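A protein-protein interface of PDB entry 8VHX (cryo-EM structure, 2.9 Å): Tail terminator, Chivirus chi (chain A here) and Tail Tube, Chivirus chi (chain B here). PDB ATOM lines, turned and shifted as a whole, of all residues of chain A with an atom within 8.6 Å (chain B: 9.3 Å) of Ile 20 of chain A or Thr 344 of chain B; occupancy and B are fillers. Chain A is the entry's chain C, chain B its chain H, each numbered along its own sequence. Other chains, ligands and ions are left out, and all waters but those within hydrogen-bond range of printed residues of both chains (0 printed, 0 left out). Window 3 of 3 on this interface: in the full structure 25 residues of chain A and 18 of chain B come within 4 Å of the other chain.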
ATOM      1  N   GLU A  16     -10.842  18.101   4.709  1.00  0.00           N
ATOM      2  CA  GLU A  16      -9.878  19.185   4.766  1.00  0.00           C
ATOM      3  C   GLU A  16      -9.670  19.703   6.173  1.00  0.00           C
ATOM      4  O   GLU A  16      -8.935  20.677   6.361  1.00  0.00           O
ATOM      5  CB  GLU A  16     -10.326  20.316   3.854  1.00  0.00           C
ATOM      6  CG  GLU A  16     -10.155  20.011   2.393  1.00  0.00           C
ATOM      7  CD  GLU A  16     -10.600  21.142   1.486  1.00  0.00           C
ATOM      8  OE1 GLU A  16     -11.572  21.841   1.830  1.00  0.00           O
ATOM      9  OE2 GLU A  16      -9.989  21.321   0.415  1.00  0.00           O
ATOM     10  N   GLN A  17     -10.317  19.089   7.152  1.00  0.00           N
ATOM     11  CA  GLN A  17     -10.103  19.365   8.558  1.00  0.00           C
ATOM     12  C   GLN A  17      -9.279  18.288   9.227  1.00  0.00           C
ATOM     13  O   GLN A  17      -9.112  18.316  10.447  1.00  0.00           O
ATOM     14  CB  GLN A  17     -11.433  19.506   9.281  1.00  0.00           C
ATOM     15  CG  GLN A  17     -12.178  20.764   8.958  1.00  0.00           C
ATOM     16  CD  GLN A  17     -13.567  20.755   9.512  1.00  0.00           C
ATOM     17  OE1 GLN A  17     -13.768  20.780  10.726  1.00  0.00           O
ATOM     18  NE2 GLN A  17     -14.545  20.697   8.624  1.00  0.00           N
ATOM     19  N   ILE A  18      -8.784  17.327   8.460  1.00  0.00           N
ATOM     20  CA  ILE A  18      -7.768  16.419   8.952  1.00  0.00           C
ATOM     21  C   ILE A  18      -6.479  17.211   8.955  1.00  0.00           C
ATOM     22  O   ILE A  18      -5.817  17.361   7.925  1.00  0.00           O
ATOM     23  CB  ILE A  18      -7.663  15.154   8.096  1.00  0.00           C
ATOM     24  CG1 ILE A  18      -8.945  14.351   8.188  1.00  0.00           C
ATOM     25  CG2 ILE A  18      -6.540  14.297   8.545  1.00  0.00           C
ATOM     26  CD1 ILE A  18      -9.057  13.326   7.151  1.00  0.00           C
ATOM     27  N   THR A  19      -6.129  17.727  10.122  1.00  0.00           N
ATOM     28  CA  THR A  19      -5.043  18.669  10.266  1.00  0.00           C
ATOM     29  C   THR A  19      -4.378  18.423  11.604  1.00  0.00           C
ATOM     30  O   THR A  19      -4.982  17.885  12.532  1.00  0.00           O
ATOM     31  CB  THR A  19      -5.547  20.107  10.166  1.00  0.00           C
ATOM     32  OG1 THR A  19      -6.504  20.204   9.112  1.00  0.00           O
ATOM     33  CG2 THR A  19      -4.423  21.048   9.868  1.00  0.00           C
ATOM     34  N   ILE A  20      -3.115  18.822  11.692  1.00  0.00           N
ATOM     35  CA  ILE A  20      -2.364  18.594  12.915  1.00  0.00           C
ATOM     36  C   ILE A  20      -2.881  19.489  14.029  1.00  0.00           C
ATOM     37  O   ILE A  20      -2.784  19.151  15.213  1.00  0.00           O
ATOM     38  CB  ILE A  20      -0.867  18.782  12.644  1.00  0.00           C
ATOM     39  CG1 ILE A  20      -0.406  17.693  11.687  1.00  0.00           C
ATOM     40  CG2 ILE A  20      -0.107  18.689  13.918  1.00  0.00           C
ATOM     41  CD1 ILE A  20       0.902  17.939  11.048  1.00  0.00           C
ATOM     42  N   ALA A  21      -3.435  20.645  13.671  1.00  0.00           N
ATOM     43  CA  ALA A  21      -4.089  21.492  14.656  1.00  0.00           C
ATOM     44  C   ALA A  21      -5.383  20.893  15.186  1.00  0.00           C
ATOM     45  O   ALA A  21      -5.879  21.347  16.220  1.00  0.00           O
ATOM     46  CB  ALA A  21      -4.370  22.861  14.061  1.00  0.00           C
ATOM     47  N   ASN A  22      -5.955  19.910  14.496  1.00  0.00           N
ATOM     48  CA  ASN A  22      -7.202  19.279  14.903  1.00  0.00           C
ATOM     49  C   ASN A  22      -6.998  17.925  15.557  1.00  0.00           C
ATOM     50  O   ASN A  22      -7.980  17.248  15.872  1.00  0.00           O
ATOM     51  CB  ASN A  22      -8.133  19.118  13.706  1.00  0.00           C
ATOM     52  CG  ASN A  22      -8.721  20.402  13.256  1.00  0.00           C
ATOM     53  OD1 ASN A  22      -8.030  21.287  12.758  1.00  0.00           O
ATOM     54  ND2 ASN A  22     -10.023  20.504  13.385  1.00  0.00           N
ATOM     55  N   GLY A  23      -5.757  17.511  15.760  1.00  0.00           N
ATOM     56  CA  GLY A  23      -5.489  16.256  16.427  1.00  0.00           C
ATOM     57  C   GLY A  23      -5.339  15.082  15.504  1.00  0.00           C
ATOM     58  O   GLY A  23      -5.658  13.952  15.884  1.00  0.00           O
ATOM     59  N   TYR A  24      -4.853  15.316  14.298  1.00  0.00           N
ATOM     60  CA  TYR A  24      -4.544  14.267  13.351  1.00  0.00           C
ATOM     61  C   TYR A  24      -3.075  14.371  12.985  1.00  0.00           C
ATOM     62  O   TYR A  24      -2.480  15.446  13.057  1.00  0.00           O
ATOM     63  CB  TYR A  24      -5.413  14.377  12.106  1.00  0.00           C
ATOM     64  CG  TYR A  24      -6.896  14.374  12.360  1.00  0.00           C
ATOM     65  CD1 TYR A  24      -7.606  13.198  12.450  1.00  0.00           C
ATOM     66  CD2 TYR A  24      -7.592  15.552  12.484  1.00  0.00           C
ATOM     67  CE1 TYR A  24      -8.950  13.200  12.671  1.00  0.00           C
ATOM     68  CE2 TYR A  24      -8.933  15.558  12.703  1.00  0.00           C
ATOM     69  CZ  TYR A  24      -9.608  14.381  12.795  1.00  0.00           C
ATOM     70  OH  TYR A  24     -10.958  14.375  13.016  1.00  0.00           O
ATOM     71  N   ALA A  25      -2.481  13.245  12.608  1.00  0.00           N
ATOM     72  CA  ALA A  25      -1.060  13.235  12.302  1.00  0.00           C
ATOM     73  C   ALA A  25      -0.746  13.718  10.900  1.00  0.00           C
ATOM     74  O   ALA A  25       0.432  13.836  10.555  1.00  0.00           O
ATOM     75  CB  ALA A  25      -0.497  11.836  12.493  1.00  0.00           C
ATOM     76  N   TYR A  26      -1.758  13.987  10.091  1.00  0.00           N
ATOM     77  CA  TYR A  26      -1.577  14.385   8.710  1.00  0.00           C
ATOM     78  C   TYR A  26      -2.360  15.659   8.455  1.00  0.00           C
ATOM     79  O   TYR A  26      -3.363  15.939   9.111  1.00  0.00           O
ATOM     80  CB  TYR A  26      -2.017  13.278   7.756  1.00  0.00           C
ATOM     81  CG  TYR A  26      -1.067  12.111   7.707  1.00  0.00           C
ATOM     82  CD1 TYR A  26       0.137  12.204   7.037  1.00  0.00           C
ATOM     83  CD2 TYR A  26      -1.359  10.927   8.350  1.00  0.00           C
ATOM     84  CE1 TYR A  26       1.007  11.152   6.993  1.00  0.00           C
ATOM     85  CE2 TYR A  26      -0.489   9.870   8.311  1.00  0.00           C
ATOM     86  CZ  TYR A  26       0.692   9.985   7.630  1.00  0.00           C
ATOM     87  OH  TYR A  26       1.575   8.934   7.583  1.00  0.00           O
ATOM     88  N   ASP A  27      -1.880  16.433   7.492  1.00  0.00           N
ATOM     89  CA  ASP A  27      -2.421  17.750   7.189  1.00  0.00           C
ATOM     90  C   ASP A  27      -2.948  17.720   5.764  1.00  0.00           C
ATOM     91  O   ASP A  27      -2.167  17.695   4.810  1.00  0.00           O
ATOM     92  CB  ASP A  27      -1.356  18.824   7.374  1.00  0.00           C
ATOM     93  CG  ASP A  27      -1.927  20.215   7.374  1.00  0.00           C
ATOM     94  OD1 ASP A  27      -3.018  20.413   6.805  1.00  0.00           O
ATOM     95  OD2 ASP A  27      -1.293  21.112   7.967  1.00  0.00           O
ATOM     96  N   LEU A  28      -4.270  17.722   5.629  1.00  0.00           N
ATOM     97  CA  LEU A  28      -4.935  17.599   4.344  1.00  0.00           C
ATOM     98  C   LEU A  28      -5.606  18.885   3.907  1.00  0.00           C
ATOM     99  O   LEU A  28      -6.331  18.888   2.910  1.00  0.00           O
ATOM    100  CB  LEU A  28      -5.968  16.485   4.395  1.00  0.00           C
ATOM    101  CG  LEU A  28      -5.455  15.056   4.349  1.00  0.00           C
ATOM    102  CD1 LEU A  28      -6.544  14.099   4.649  1.00  0.00           C
ATOM    103  CD2 LEU A  28      -4.953  14.775   3.005  1.00  0.00           C
ATOM    104  N   LYS A  29      -5.390  19.973   4.624  1.00  0.00           N
ATOM    105  CA  LYS A  29      -6.039  21.222   4.279  1.00  0.00           C
ATOM    106  C   LYS A  29      -5.583  21.682   2.907  1.00  0.00           C
ATOM    107  O   LYS A  29      -4.382  21.794   2.644  1.00  0.00           O
ATOM    108  CB  LYS A  29      -5.739  22.277   5.326  1.00  0.00           C
ATOM    109  CG  LYS A  29      -6.515  23.544   5.131  1.00  0.00           C
ATOM    110  CD  LYS A  29      -6.322  24.498   6.284  1.00  0.00           C
ATOM    111  CE  LYS A  29      -7.179  25.730   6.117  1.00  0.00           C
ATOM    112  NZ  LYS A  29      -7.036  26.681   7.255  1.00  0.00           N
ATOM    113  N   PRO A  48       0.702  14.368   1.836  1.00  0.00           N
ATOM    114  CA  PRO A  48      -0.392  13.478   1.441  1.00  0.00           C
ATOM    115  C   PRO A  48      -1.514  14.193   0.715  1.00  0.00           C
ATOM    116  O   PRO A  48      -1.748  15.368   0.955  1.00  0.00           O
ATOM    117  CB  PRO A  48      -0.881  12.930   2.775  1.00  0.00           C
ATOM    118  CG  PRO A  48      -0.628  14.020   3.718  1.00  0.00           C
ATOM    119  CD  PRO A  48       0.636  14.692   3.269  1.00  0.00           C
ATOM    120  N   THR B 308      -2.761   8.810  24.762  1.00  0.00           N
ATOM    121  CA  THR B 308      -3.112  10.124  24.242  1.00  0.00           C
ATOM    122  C   THR B 308      -4.621  10.288  24.228  1.00  0.00           C
ATOM    123  O   THR B 308      -5.346   9.395  23.774  1.00  0.00           O
ATOM    124  CB  THR B 308      -2.549  10.328  22.839  1.00  0.00           C
ATOM    125  OG1 THR B 308      -1.150  10.035  22.837  1.00  0.00           O
ATOM    126  CG2 THR B 308      -2.751  11.753  22.401  1.00  0.00           C
ATOM    127  N   VAL B 309      -5.083  11.421  24.741  1.00  0.00           N
ATOM    128  CA  VAL B 309      -6.497  11.758  24.801  1.00  0.00           C
ATOM    129  C   VAL B 309      -6.737  12.919  23.855  1.00  0.00           C
ATOM    130  O   VAL B 309      -5.944  13.864  23.816  1.00  0.00           O
ATOM    131  CB  VAL B 309      -6.924  12.125  26.228  1.00  0.00           C
ATOM    132  CG1 VAL B 309      -6.363  13.461  26.599  1.00  0.00           C
ATOM    133  CG2 VAL B 309      -8.414  12.135  26.344  1.00  0.00           C
ATOM    134  N   THR B 310      -7.815  12.844  23.089  1.00  0.00           N
ATOM    135  CA  THR B 310      -8.200  13.905  22.175  1.00  0.00           C
ATOM    136  C   THR B 310      -9.611  14.353  22.513  1.00  0.00           C
ATOM    137  O   THR B 310     -10.519  13.526  22.626  1.00  0.00           O
ATOM    138  CB  THR B 310      -8.119  13.436  20.721  1.00  0.00           C
ATOM    139  OG1 THR B 310      -6.918  12.679  20.528  1.00  0.00           O
ATOM    140  CG2 THR B 310      -8.085  14.610  19.792  1.00  0.00           C
ATOM    141  N   VAL B 311      -9.787  15.659  22.675  1.00  0.00           N
ATOM    142  CA  VAL B 311     -11.064  16.249  23.045  1.00  0.00           C
ATOM    143  C   VAL B 311     -11.573  17.080  21.883  1.00  0.00           C
ATOM    144  O   VAL B 311     -10.835  17.897  21.323  1.00  0.00           O
ATOM    145  CB  VAL B 311     -10.934  17.103  24.310  1.00  0.00           C
ATOM    146  CG1 VAL B 311     -12.269  17.590  24.732  1.00  0.00           C
ATOM    147  CG2 VAL B 311     -10.316  16.291  25.395  1.00  0.00           C
ATOM    148  N   ARG B 312     -12.836  16.876  21.529  1.00  0.00           N
ATOM    149  CA  ARG B 312     -13.439  17.505  20.371  1.00  0.00           C
ATOM    150  C   ARG B 312     -14.823  18.019  20.720  1.00  0.00           C
ATOM    151  O   ARG B 312     -15.493  17.488  21.607  1.00  0.00           O
ATOM    152  CB  ARG B 312     -13.544  16.532  19.220  1.00  0.00           C
ATOM    153  CG  ARG B 312     -12.255  15.949  18.782  1.00  0.00           C
ATOM    154  CD  ARG B 312     -12.447  15.082  17.592  1.00  0.00           C
ATOM    155  NE  ARG B 312     -11.216  14.414  17.210  1.00  0.00           N
ATOM    156  CZ  ARG B 312     -10.207  15.012  16.599  1.00  0.00           C
ATOM    157  NH1 ARG B 312      -9.126  14.328  16.298  1.00  0.00           N
ATOM    158  NH2 ARG B 312     -10.288  16.283  16.273  1.00  0.00           N
ATOM    159  N   GLY B 316     -16.489  18.224  15.529  1.00  0.00           N
ATOM    160  CA  GLY B 316     -15.268  17.497  15.322  1.00  0.00           C
ATOM    161  C   GLY B 316     -14.017  18.303  15.552  1.00  0.00           C
ATOM    162  O   GLY B 316     -12.915  17.750  15.462  1.00  0.00           O
ATOM    163  N   THR B 317     -14.152  19.587  15.850  1.00  0.00           N
ATOM    164  CA  THR B 317     -12.997  20.437  16.066  1.00  0.00           C
ATOM    165  C   THR B 317     -12.355  20.143  17.408  1.00  0.00           C
ATOM    166  O   THR B 317     -13.029  19.804  18.381  1.00  0.00           O
ATOM    167  CB  THR B 317     -13.402  21.898  15.997  1.00  0.00           C
ATOM    168  OG1 THR B 317     -14.056  22.157  14.751  1.00  0.00           O
ATOM    169  CG2 THR B 317     -12.193  22.775  16.109  1.00  0.00           C
ATOM    170  N   ALA B 318     -11.039  20.283  17.447  1.00  0.00           N
ATOM    171  CA  ALA B 318     -10.286  20.040  18.663  1.00  0.00           C
ATOM    172  C   ALA B 318     -10.439  21.205  19.622  1.00  0.00           C
ATOM    173  O   ALA B 318     -10.459  22.369  19.216  1.00  0.00           O
ATOM    174  CB  ALA B 318      -8.827  19.830  18.331  1.00  0.00           C
ATOM    175  N   VAL B 319     -10.547  20.887  20.904  1.00  0.00           N
ATOM    176  CA  VAL B 319     -10.836  21.870  21.933  1.00  0.00           C
ATOM    177  C   VAL B 319      -9.548  22.199  22.668  1.00  0.00           C
ATOM    178  O   VAL B 319      -8.963  21.341  23.335  1.00  0.00           O
ATOM    179  CB  VAL B 319     -11.899  21.363  22.902  1.00  0.00           C
ATOM    180  CG1 VAL B 319     -12.160  22.406  23.929  1.00  0.00           C
ATOM    181  CG2 VAL B 319     -13.133  21.031  22.159  1.00  0.00           C
ATOM    182  N   GLN B 320      -9.107  23.443  22.542  1.00  0.00           N
ATOM    183  CA  GLN B 320      -8.003  23.931  23.349  1.00  0.00           C
ATOM    184  C   GLN B 320      -8.505  24.336  24.729  1.00  0.00           C
ATOM    185  O   GLN B 320      -9.473  25.091  24.857  1.00  0.00           O
ATOM    186  CB  GLN B 320      -7.335  25.106  22.634  1.00  0.00           C
ATOM    187  CG  GLN B 320      -6.555  26.084  23.510  1.00  0.00           C
ATOM    188  CD  GLN B 320      -5.351  25.452  24.174  1.00  0.00           C
ATOM    189  OE1 GLN B 320      -4.589  24.733  23.536  1.00  0.00           O
ATOM    190  NE2 GLN B 320      -5.173  25.717  25.457  1.00  0.00           N
ATOM    191  N   GLY B 321      -7.850  23.822  25.768  1.00  0.00           N
ATOM    192  CA  GLY B 321      -8.079  24.309  27.111  1.00  0.00           C
ATOM    193  C   GLY B 321      -9.127  23.595  27.934  1.00  0.00           C
ATOM    194  O   GLY B 321      -9.675  24.208  28.856  1.00  0.00           O
ATOM    195  N   THR B 340      -4.451  19.766  31.001  1.00  0.00           N
ATOM    196  CA  THR B 340      -5.220  20.666  30.161  1.00  0.00           C
ATOM    197  C   THR B 340      -4.835  20.417  28.712  1.00  0.00           C
ATOM    198  O   THR B 340      -3.649  20.274  28.396  1.00  0.00           O
ATOM    199  CB  THR B 340      -4.969  22.122  30.546  1.00  0.00           C
ATOM    200  OG1 THR B 340      -5.453  22.350  31.872  1.00  0.00           O
ATOM    201  CG2 THR B 340      -5.672  23.056  29.592  1.00  0.00           C
ATOM    202  N   THR B 341      -5.834  20.359  27.841  1.00  0.00           N
ATOM    203  CA  THR B 341      -5.591  19.980  26.458  1.00  0.00           C
ATOM    204  C   THR B 341      -4.843  21.073  25.712  1.00  0.00           C
ATOM    205  O   THR B 341      -5.096  22.266  25.896  1.00  0.00           O
ATOM    206  CB  THR B 341      -6.907  19.674  25.758  1.00  0.00           C
ATOM    207  OG1 THR B 341      -7.788  20.795  25.869  1.00  0.00           O
ATOM    208  CG2 THR B 341      -7.551  18.470  26.369  1.00  0.00           C
ATOM    209  N   GLY B 342      -3.917  20.650  24.860  1.00  0.00           N
ATOM    210  CA  GLY B 342      -3.170  21.566  24.032  1.00  0.00           C
ATOM    211  C   GLY B 342      -3.985  22.117  22.888  1.00  0.00           C
ATOM    212  O   GLY B 342      -5.174  21.852  22.732  1.00  0.00           O
ATOM    213  N   ALA B 343      -3.309  22.915  22.059  1.00  0.00           N
ATOM    214  CA  ALA B 343      -3.981  23.534  20.924  1.00  0.00           C
ATOM    215  C   ALA B 343      -4.570  22.484  20.001  1.00  0.00           C
ATOM    216  O   ALA B 343      -5.639  22.690  19.418  1.00  0.00           O
ATOM    217  CB  ALA B 343      -3.003  24.414  20.158  1.00  0.00           C
ATOM    218  N   THR B 344      -3.892  21.356  19.867  1.00  0.00           N
ATOM    219  CA  THR B 344      -4.361  20.249  19.056  1.00  0.00           C
ATOM    220  C   THR B 344      -5.388  19.396  19.773  1.00  0.00           C
ATOM    221  O   THR B 344      -5.677  18.286  19.320  1.00  0.00           O
ATOM    222  CB  THR B 344      -3.174  19.392  18.634  1.00  0.00           C
ATOM    223  OG1 THR B 344      -2.527  18.861  19.794  1.00  0.00           O
ATOM    224  CG2 THR B 344      -2.192  20.230  17.878  1.00  0.00           C
ATOM    225  N   GLY B 345      -5.925  19.878  20.886  1.00  0.00           N
ATOM    226  CA  GLY B 345      -6.941  19.160  21.626  1.00  0.00           C
ATOM    227  C   GLY B 345      -6.455  17.886  22.268  1.00  0.00           C
ATOM    228  O   GLY B 345      -7.248  17.127  22.827  1.00  0.00           O
ATOM    229  N   THR B 346      -5.159  17.636  22.195  1.00  0.00           N
ATOM    230  CA  THR B 346      -4.593  16.428  22.761  1.00  0.00           C
ATOM    231  C   THR B 346      -3.987  16.704  24.129  1.00  0.00           C
ATOM    232  O   THR B 346      -3.555  17.817  24.436  1.00  0.00           O
ATOM    233  CB  THR B 346      -3.529  15.844  21.835  1.00  0.00           C
ATOM    234  OG1 THR B 346      -2.562  16.847  21.522  1.00  0.00           O
ATOM    235  CG2 THR B 346      -4.153  15.324  20.547  1.00  0.00           C
ATOM    236  N   ALA B 347      -3.977  15.666  24.958  1.00  0.00           N
ATOM    237  CA  ALA B 347      -3.162  15.628  26.158  1.00  0.00           C
ATOM    238  C   ALA B 347      -2.579  14.235  26.298  1.00  0.00           C
ATOM    239  O   ALA B 347      -3.118  13.256  25.777  1.00  0.00           O
ATOM    240  CB  ALA B 347      -3.947  15.987  27.416  1.00  0.00           C
ATOM    241  N   THR B 348      -1.465  14.157  27.008  1.00  0.00           N
ATOM    242  CA  THR B 348      -0.784  12.899  27.246  1.00  0.00           C
ATOM    243  C   THR B 348      -0.408  12.789  28.712  1.00  0.00           C
ATOM    244  O   THR B 348      -0.116  13.789  29.372  1.00  0.00           O
ATOM    245  CB  THR B 348       0.463  12.781  26.384  1.00  0.00           C
ATOM    246  OG1 THR B 348       1.319  13.901  26.631  1.00  0.00           O
ATOM    247  CG2 THR B 348       0.086  12.753  24.923  1.00  0.00           C
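Of chain B, only Thr 344 (2.9 Å) comes within 4 Å of Ile 20 of chain A. Of the printed residues of chain A, Thr 344 of chain B touches Ile 20 (2.9 Å), Ala 21 (3.4 Å) and Gly 23 (3.5 Å). No residue of chain B comes within 4 Å of Thr 19 of chain A. Ala 21 of chain A touches just these residues of chain B: Ala 318 (3.9 Å), Ala 343 (3.5 Å) and Thr 344 (3.4 Å). No residue of chain A comes within 4 Å of Gly 345 of chain B. Of the printed residues of chain B, Gly 23 of chain A touches Arg 312 and Thr 344. Printed residues of chain B within 4 Å of Asn 22 of chain A: Arg 312 and Ala 318. Of the printed residues of chain A, Ala 318 of chain B touches Ala 21 (3.9 Å) and Asn 22 (3.7 Å). Gln 320 of chain B touches none of the printed residues of chain A. The nearest printed residue of chain A that does not touch Thr 344 of chain B is Asn 22 of chain A (4.004 Å).
O of Asn 22 of chain A sits at hydrogen-bond distance from NH2 of Arg 312 of chain B (2.5 Å). O of Ala 21 of chain A lies close to O of Ala 343 of chain B, at 3.5 Å.
Ile 20 of chain A touches Thr 344 of chain B (O to CG2, 2.9 Å). Ala 21 of chain A touches Ala 318 of chain B. CA of Thr 344 of chain B touches O of Ala 21 of chain A, at 3.4 Å. Asn 22 of chain A touches Ala 318 of chain B (O to CB, 3.7 Å). Gly 23 of chain A touches Arg 312 of chain B (O to NH1, 3.5 Å). Gly 23 of chain A touches Thr 344 of chain B. Tyr 24 of chain A touches Arg 312 of chain B (CZ to NH1, 3.5 Å).
Along chain B the printed residues that touch a printed residue of chain A span positions 312 to 344. Hydrophobic or aromatic side chains of chain A that line the printed part of chain B: Tyr 24.
The backbone NH of Tyr 24 of chain A lies within hydrogen-bond range of the backbone carbonyl oxygen of Thr 19 of chain A, at 3.1 Å. NH2 of Arg 312 of chain B lies within hydrogen-bond range of O of Gly 316 of chain B, at 3.1 Å. The side-chain amide oxygen of Gln 320 of chain B lies within hydrogen-bond range of the backbone NH of Ala 343 of chain B (2.7 Å). OG1 of Thr 344 of chain B sits at hydrogen-bond distance from OG1 of Thr 346 of chain B, 2.7 Å away.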
